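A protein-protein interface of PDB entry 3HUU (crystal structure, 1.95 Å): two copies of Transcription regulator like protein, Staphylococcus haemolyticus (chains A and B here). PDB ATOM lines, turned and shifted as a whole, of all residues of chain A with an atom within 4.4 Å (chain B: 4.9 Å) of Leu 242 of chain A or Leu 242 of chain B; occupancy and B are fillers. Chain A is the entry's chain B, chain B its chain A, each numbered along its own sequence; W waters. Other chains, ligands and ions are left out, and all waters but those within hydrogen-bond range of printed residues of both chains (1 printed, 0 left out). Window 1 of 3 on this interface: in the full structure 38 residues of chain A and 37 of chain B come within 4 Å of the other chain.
Water W1 bridges the backbone carbonyl oxygen of Asn 245 of chain B (2.6 Å) and the backbone carbonyl oxygen of Met 215 of chain A (2.8 Å).
Met 212 of chain A touches Phe 241 of chain B, and with the chains exchanged Phe 241 of chain A touches Met 212 of chain B. Met 215 of chain A touches Leu 242 of chain B, and with the chains exchanged Leu 242 of chain A touches Met 215 of chain B. Met 215 of chain A touches Asn 245 of chain B, and with the chains exchanged Asn 245 of chain A touches Met 215 of chain B. Leu 242 of chain A touches its own counterpart, Leu 242 of chain B. Positions printed for both chains: 40, 212, 215, 240, 241, 242, 243, 244, 245 and 246. Of the 10 pairs that touch across the chains among the printed residues, 7 have their exchanged pair printed and touching as well.
Among the printed residues, pairs that only touch across the chains: Pro 40 of chain A with Gln 38 of chain B, Met 212 of chain A with Phe 241 of chain B, Met 215 of chain A with Leu 242 of chain B, Ser 240 of chain A with Gln 38 of chain B, Phe 241 of chain A with Met 212 of chain B, Leu 242 of chain A with Met 215 of chain B and Leu 242 of chain A with Leu 242 of chain B.
The backbone carbonyl oxygen (O) of Phe 241 of chain A lies within hydrogen-bond range of the side-chain amide nitrogen (ND2) of Asn 245 of chain A, at 3.0 Å. OG of Ser 240 of chain A lies close to N of Leu 242 of chain A (3.3 Å). OG1 of Thr 243 of chain A lies within hydrogen-bond range of O of Ser 240 of chain A (3.1 Å). O of Phe 241 of chain B lies within hydrogen-bond range of ND2 of Asn 245 of chain B (2.9 Å).
Of the 11 printed residues of chain B, 6 touch a printed residue of chain A. Among the printed residues, 10 pairs touch across the chains. Among the printed residues, no Asp or Glu carboxylate lies within 4 Å of a Lys or Arg side-chain nitrogen of the other chain.
Of the printed residues of chain B, Met 215 of chain A touches Leu 242 (3.4 Å) and Asn 245 (3.4 Å). Of the printed residues of chain B, Phe 241 of chain A touches Gln 38 and Met 212. Printed residues of chain A within 4 Å of Gln 38 of chain B: Pro 40 (3.9 Å), Ser 240 (3.5 Å) and Phe 241 (2.9 Å). Printed residues of chain A within 4 Å of Met 212 of chain B: Phe 241 (3.5 Å). Of the printed residues of chain A, Leu 242 of chain B touches Met 215 (3.4 Å) and Leu 242 (3.4 Å).
The backbone NH of Phe 241 of chain A lies within hydrogen-bond range of the side-chain amide oxygen of Gln 38 of chain B, at 2.9 Å. The backbone carbonyl oxygen of Asn 245 of chain B sits close to the backbone carbonyl oxygen of Met 215 of chain A (3.4 Å). O of Asn 245 of chain A lies close to O of Met 215 of chain B (3.4 Å).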
ATOM      1  N   PRO A  40     -18.150  23.780 -14.902  1.00  0.00           N
ATOM      2  CA  PRO A  40     -16.932  23.392 -14.179  1.00  0.00           C
ATOM      3  C   PRO A  40     -16.689  24.257 -12.948  1.00  0.00           C
ATOM      4  O   PRO A  40     -16.089  23.810 -11.972  1.00  0.00           O
ATOM      5  CB  PRO A  40     -15.841  23.571 -15.232  1.00  0.00           C
ATOM      6  CG  PRO A  40     -16.553  23.253 -16.494  1.00  0.00           C
ATOM      7  CD  PRO A  40     -17.863  23.974 -16.336  1.00  0.00           C
ATOM      8  N   VAL A 211     -17.928  29.960 -19.896  1.00  0.00           N
ATOM      9  CA  VAL A 211     -17.606  28.770 -20.674  1.00  0.00           C
ATOM     10  C   VAL A 211     -18.792  28.007 -21.287  1.00  0.00           C
ATOM     11  O   VAL A 211     -18.675  27.471 -22.393  1.00  0.00           O
ATOM     12  CB  VAL A 211     -16.763  27.789 -19.818  1.00  0.00           C
ATOM     13  CG1 VAL A 211     -17.605  27.214 -18.691  1.00  0.00           C
ATOM     14  CG2 VAL A 211     -16.198  26.689 -20.691  1.00  0.00           C
ATOM     15  N   MET A 212     -19.923  27.953 -20.588  1.00  0.00           N
ATOM     16  CA  MET A 212     -21.081  27.232 -21.124  1.00  0.00           C
ATOM     17  C   MET A 212     -21.637  27.972 -22.358  1.00  0.00           C
ATOM     18  O   MET A 212     -21.983  27.350 -23.375  1.00  0.00           O
ATOM     19  CB  MET A 212     -22.146  27.037 -20.030  1.00  0.00           C
ATOM     20  CG  MET A 212     -21.643  26.201 -18.816  1.00  0.00           C
ATOM     21  SD  MET A 212     -20.834  24.616 -19.178  1.00  0.00           S
ATOM     22  CE  MET A 212     -22.046  23.471 -18.431  1.00  0.00           C
ATOM     23  N   MET A 215     -19.311  27.267 -25.231  1.00  0.00           N
ATOM     24  CA  MET A 215     -19.508  25.991 -25.926  1.00  0.00           C
ATOM     25  C   MET A 215     -20.562  26.150 -27.023  1.00  0.00           C
ATOM     26  O   MET A 215     -20.427  25.623 -28.130  1.00  0.00           O
ATOM     27  CB  MET A 215     -19.962  24.884 -24.952  1.00  0.00           C
ATOM     28  CG  MET A 215     -18.863  24.310 -24.046  1.00  0.00           C
ATOM     29  SD  MET A 215     -19.360  22.725 -23.252  1.00  0.00           S
ATOM     30  CE  MET A 215     -19.163  21.605 -24.634  1.00  0.00           C
ATOM     31  N   SER A 240     -10.726  25.458 -17.553  1.00  0.00           N
ATOM     32  CA  SER A 240     -11.101  24.140 -17.067  1.00  0.00           C
ATOM     33  C   SER A 240     -10.888  23.135 -18.191  1.00  0.00           C
ATOM     34  O   SER A 240     -10.426  23.496 -19.275  1.00  0.00           O
ATOM     35  CB  SER A 240     -12.573  24.135 -16.678  1.00  0.00           C
ATOM     36  OG  SER A 240     -13.358  24.385 -17.831  1.00  0.00           O
ATOM     37  N   PHE A 241     -11.247  21.881 -17.942  1.00  0.00           N
ATOM     38  CA  PHE A 241     -11.097  20.837 -18.947  1.00  0.00           C
ATOM     39  C   PHE A 241     -11.863  21.230 -20.202  1.00  0.00           C
ATOM     40  O   PHE A 241     -11.449  20.919 -21.325  1.00  0.00           O
ATOM     41  CB  PHE A 241     -11.646  19.505 -18.417  1.00  0.00           C
ATOM     42  CG  PHE A 241     -11.314  18.324 -19.287  1.00  0.00           C
ATOM     43  CD1 PHE A 241     -10.112  17.630 -19.118  1.00  0.00           C
ATOM     44  CD2 PHE A 241     -12.195  17.905 -20.280  1.00  0.00           C
ATOM     45  CE1 PHE A 241      -9.801  16.529 -19.935  1.00  0.00           C
ATOM     46  CE2 PHE A 241     -11.895  16.812 -21.100  1.00  0.00           C
ATOM     47  CZ  PHE A 241     -10.697  16.122 -20.926  1.00  0.00           C
ATOM     48  N   LEU A 242     -12.985  21.910 -20.010  1.00  0.00           N
ATOM     49  CA  LEU A 242     -13.807  22.327 -21.135  1.00  0.00           C
ATOM     50  C   LEU A 242     -13.127  23.339 -22.051  1.00  0.00           C
ATOM     51  O   LEU A 242     -13.273  23.257 -23.273  1.00  0.00           O
ATOM     52  CB  LEU A 242     -15.135  22.911 -20.651  1.00  0.00           C
ATOM     53  CG  LEU A 242     -15.998  22.033 -19.740  1.00  0.00           C
ATOM     54  CD1 LEU A 242     -17.447  22.516 -19.855  1.00  0.00           C
ATOM     55  CD2 LEU A 242     -15.894  20.575 -20.122  1.00  0.00           C
ATOM     56  N   THR A 243     -12.395  24.297 -21.483  1.00  0.00           N
ATOM     57  CA  THR A 243     -11.724  25.287 -22.330  1.00  0.00           C
ATOM     58  C   THR A 243     -10.452  24.698 -22.936  1.00  0.00           C
ATOM     59  O   THR A 243     -10.132  24.967 -24.089  1.00  0.00           O
ATOM     60  CB  THR A 243     -11.351  26.585 -21.550  1.00  0.00           C
ATOM     61  OG1 THR A 243     -10.377  26.292 -20.542  1.00  0.00           O
ATOM     62  CG2 THR A 243     -12.586  27.183 -20.881  1.00  0.00           C
ATOM     63  N   GLU A 244      -9.737  23.882 -22.165  1.00  0.00           N
ATOM     64  CA  GLU A 244      -8.501  23.266 -22.644  1.00  0.00           C
ATOM     65  C   GLU A 244      -8.735  22.263 -23.767  1.00  0.00           C
ATOM     66  O   GLU A 244      -7.894  22.104 -24.669  1.00  0.00           O
ATOM     67  CB  GLU A 244      -7.783  22.547 -21.498  1.00  0.00           C
ATOM     68  CG  GLU A 244      -7.325  23.443 -20.355  1.00  0.00           C
ATOM     69  CD  GLU A 244      -6.220  24.399 -20.766  1.00  0.00           C
ATOM     70  OE1 GLU A 244      -6.494  25.334 -21.551  1.00  0.00           O
ATOM     71  OE2 GLU A 244      -5.071  24.212 -20.305  1.00  0.00           O
ATOM     72  N   ASN A 245      -9.875  21.577 -23.712  1.00  0.00           N
ATOM     73  CA  ASN A 245     -10.198  20.578 -24.717  1.00  0.00           C
ATOM     74  C   ASN A 245     -11.358  20.973 -25.613  1.00  0.00           C
ATOM     75  O   ASN A 245     -11.981  20.119 -26.235  1.00  0.00           O
ATOM     76  CB  ASN A 245     -10.489  19.244 -24.026  1.00  0.00           C
ATOM     77  CG  ASN A 245      -9.281  18.709 -23.276  1.00  0.00           C
ATOM     78  OD1 ASN A 245      -8.415  18.065 -23.859  1.00  0.00           O
ATOM     79  ND2 ASN A 245      -9.211  18.997 -21.979  1.00  0.00           N
ATOM     80  N   ALA A 246     -11.646  22.268 -25.682  1.00  0.00           N
ATOM     81  CA  ALA A 246     -12.725  22.755 -26.532  1.00  0.00           C
ATOM     82  C   ALA A 246     -12.294  22.609 -27.986  1.00  0.00           C
ATOM     83  O   ALA A 246     -11.180  22.169 -28.272  1.00  0.00           O
ATOM     84  CB  ALA A 246     -13.025  24.217 -26.222  1.00  0.00           C
ATOM     85  N   GLN B  38     -14.847  17.260 -13.045  1.00  0.00           N
ATOM     86  CA  GLN B  38     -15.598  18.113 -13.957  1.00  0.00           C
ATOM     87  C   GLN B  38     -16.532  17.353 -14.899  1.00  0.00           C
ATOM     88  O   GLN B  38     -17.335  17.965 -15.608  1.00  0.00           O
ATOM     89  CB  GLN B  38     -14.633  19.011 -14.743  1.00  0.00           C
ATOM     90  CG  GLN B  38     -14.165  20.209 -13.920  1.00  0.00           C
ATOM     91  CD  GLN B  38     -12.982  20.942 -14.540  1.00  0.00           C
ATOM     92  OE1 GLN B  38     -12.696  20.792 -15.722  1.00  0.00           O
ATOM     93  NE2 GLN B  38     -12.301  21.754 -13.736  1.00  0.00           N
ATOM     94  N   PRO B  40     -19.645  15.809 -16.172  1.00  0.00           N
ATOM     95  CA  PRO B  40     -21.027  16.077 -15.771  1.00  0.00           C
ATOM     96  C   PRO B  40     -21.747  14.900 -15.104  1.00  0.00           C
ATOM     97  O   PRO B  40     -22.767  15.090 -14.446  1.00  0.00           O
ATOM     98  CB  PRO B  40     -21.687  16.529 -17.075  1.00  0.00           C
ATOM     99  CG  PRO B  40     -20.891  15.830 -18.127  1.00  0.00           C
ATOM    100  CD  PRO B  40     -19.474  15.997 -17.625  1.00  0.00           C
ATOM    101  N   MET B 212     -15.743  13.006 -21.699  1.00  0.00           N
ATOM    102  CA  MET B 212     -14.504  13.776 -21.585  1.00  0.00           C
ATOM    103  C   MET B 212     -13.494  13.288 -22.634  1.00  0.00           C
ATOM    104  O   MET B 212     -12.817  14.095 -23.274  1.00  0.00           O
ATOM    105  CB  MET B 212     -13.958  13.704 -20.147  1.00  0.00           C
ATOM    106  CG  MET B 212     -14.928  14.199 -19.077  1.00  0.00           C
ATOM    107  SD  MET B 212     -15.578  15.891 -19.331  1.00  0.00           S
ATOM    108  CE  MET B 212     -14.715  16.832 -18.087  1.00  0.00           C
ATOM    109  N   MET B 215     -14.632  14.840 -25.847  1.00  0.00           N
ATOM    110  CA  MET B 215     -14.258  16.242 -26.064  1.00  0.00           C
ATOM    111  C   MET B 215     -12.862  16.299 -26.693  1.00  0.00           C
ATOM    112  O   MET B 215     -12.607  17.069 -27.625  1.00  0.00           O
ATOM    113  CB  MET B 215     -14.232  17.042 -24.748  1.00  0.00           C
ATOM    114  CG  MET B 215     -15.586  17.441 -24.174  1.00  0.00           C
ATOM    115  SD  MET B 215     -15.474  18.810 -22.945  1.00  0.00           S
ATOM    116  CE  MET B 215     -15.420  20.238 -24.050  1.00  0.00           C
ATOM    117  N   SER B 240     -25.427  15.096 -22.007  1.00  0.00           N
ATOM    118  CA  SER B 240     -25.318  16.223 -21.088  1.00  0.00           C
ATOM    119  C   SER B 240     -25.160  17.512 -21.878  1.00  0.00           C
ATOM    120  O   SER B 240     -25.130  17.496 -23.101  1.00  0.00           O
ATOM    121  CB  SER B 240     -24.089  16.043 -20.189  1.00  0.00           C
ATOM    122  OG  SER B 240     -22.930  15.896 -20.988  1.00  0.00           O
ATOM    123  N   PHE B 241     -25.048  18.628 -21.173  1.00  0.00           N
ATOM    124  CA  PHE B 241     -24.867  19.908 -21.840  1.00  0.00           C
ATOM    125  C   PHE B 241     -23.671  19.815 -22.784  1.00  0.00           C
ATOM    126  O   PHE B 241     -23.704  20.351 -23.896  1.00  0.00           O
ATOM    127  CB  PHE B 241     -24.607  21.007 -20.814  1.00  0.00           C
ATOM    128  CG  PHE B 241     -24.650  22.389 -21.392  1.00  0.00           C
ATOM    129  CD1 PHE B 241     -25.867  23.045 -21.571  1.00  0.00           C
ATOM    130  CD2 PHE B 241     -23.473  23.029 -21.782  1.00  0.00           C
ATOM    131  CE1 PHE B 241     -25.911  24.323 -22.127  1.00  0.00           C
ATOM    132  CE2 PHE B 241     -23.503  24.304 -22.339  1.00  0.00           C
ATOM    133  CZ  PHE B 241     -24.721  24.952 -22.513  1.00  0.00           C
ATOM    134  N   LEU B 242     -22.619  19.138 -22.329  1.00  0.00           N
ATOM    135  CA  LEU B 242     -21.391  18.973 -23.106  1.00  0.00           C
ATOM    136  C   LEU B 242     -21.577  18.176 -24.397  1.00  0.00           C
ATOM    137  O   LEU B 242     -20.830  18.371 -25.354  1.00  0.00           O
ATOM    138  CB  LEU B 242     -20.300  18.287 -22.265  1.00  0.00           C
ATOM    139  CG  LEU B 242     -19.973  18.834 -20.873  1.00  0.00           C
ATOM    140  CD1 LEU B 242     -18.638  18.240 -20.402  1.00  0.00           C
ATOM    141  CD2 LEU B 242     -19.900  20.347 -20.903  1.00  0.00           C
ATOM    142  N   THR B 243     -22.539  17.258 -24.424  1.00  0.00           N
ATOM    143  CA  THR B 243     -22.762  16.490 -25.645  1.00  0.00           C
ATOM    144  C   THR B 243     -23.749  17.250 -26.523  1.00  0.00           C
ATOM    145  O   THR B 243     -23.582  17.311 -27.735  1.00  0.00           O
ATOM    146  CB  THR B 243     -23.317  15.065 -25.361  1.00  0.00           C
ATOM    147  OG1 THR B 243     -24.570  15.159 -24.679  1.00  0.00           O
ATOM    148  CG2 THR B 243     -22.336  14.267 -24.518  1.00  0.00           C
ATOM    149  N   GLU B 244     -24.765  17.849 -25.907  1.00  0.00           N
ATOM    150  CA  GLU B 244     -25.770  18.610 -26.658  1.00  0.00           C
ATOM    151  C   GLU B 244     -25.169  19.864 -27.299  1.00  0.00           C
ATOM    152  O   GLU B 244     -25.633  20.330 -28.346  1.00  0.00           O
ATOM    153  CB  GLU B 244     -26.913  19.035 -25.737  1.00  0.00           C
ATOM    154  CG  GLU B 244     -27.692  17.881 -25.103  1.00  0.00           C
ATOM    155  CD  GLU B 244     -28.483  17.063 -26.116  1.00  0.00           C
ATOM    156  OE1 GLU B 244     -27.868  16.319 -26.917  1.00  0.00           O
ATOM    157  OE2 GLU B 244     -29.727  17.168 -26.102  1.00  0.00           O
ATOM    158  N   ASN B 245     -24.131  20.407 -26.677  1.00  0.00           N
ATOM    159  CA  ASN B 245     -23.505  21.620 -27.200  1.00  0.00           C
ATOM    160  C   ASN B 245     -22.068  21.423 -27.644  1.00  0.00           C
ATOM    161  O   ASN B 245     -21.273  22.370 -27.676  1.00  0.00           O
ATOM    162  CB  ASN B 245     -23.607  22.727 -26.153  1.00  0.00           C
ATOM    163  CG  ASN B 245     -25.047  23.038 -25.797  1.00  0.00           C
ATOM    164  OD1 ASN B 245     -25.727  23.793 -26.502  1.00  0.00           O
ATOM    165  ND2 ASN B 245     -25.537  22.425 -24.720  1.00  0.00           N
ATOM    166  N   ALA B 246     -21.737  20.186 -27.989  1.00  0.00           N
ATOM    167  CA  ALA B 246     -20.402  19.882 -28.472  1.00  0.00           C
ATOM    168  C   ALA B 246     -20.303  20.429 -29.895  1.00  0.00           C
ATOM    169  O   ALA B 246     -21.280  20.944 -30.442  1.00  0.00           O
ATOM    170  CB  ALA B 246     -20.162  18.368 -28.464  1.00  0.00           C
HETATM  171  O   HOH W   1     -18.969  23.283 -28.297  1.00  0.00           O
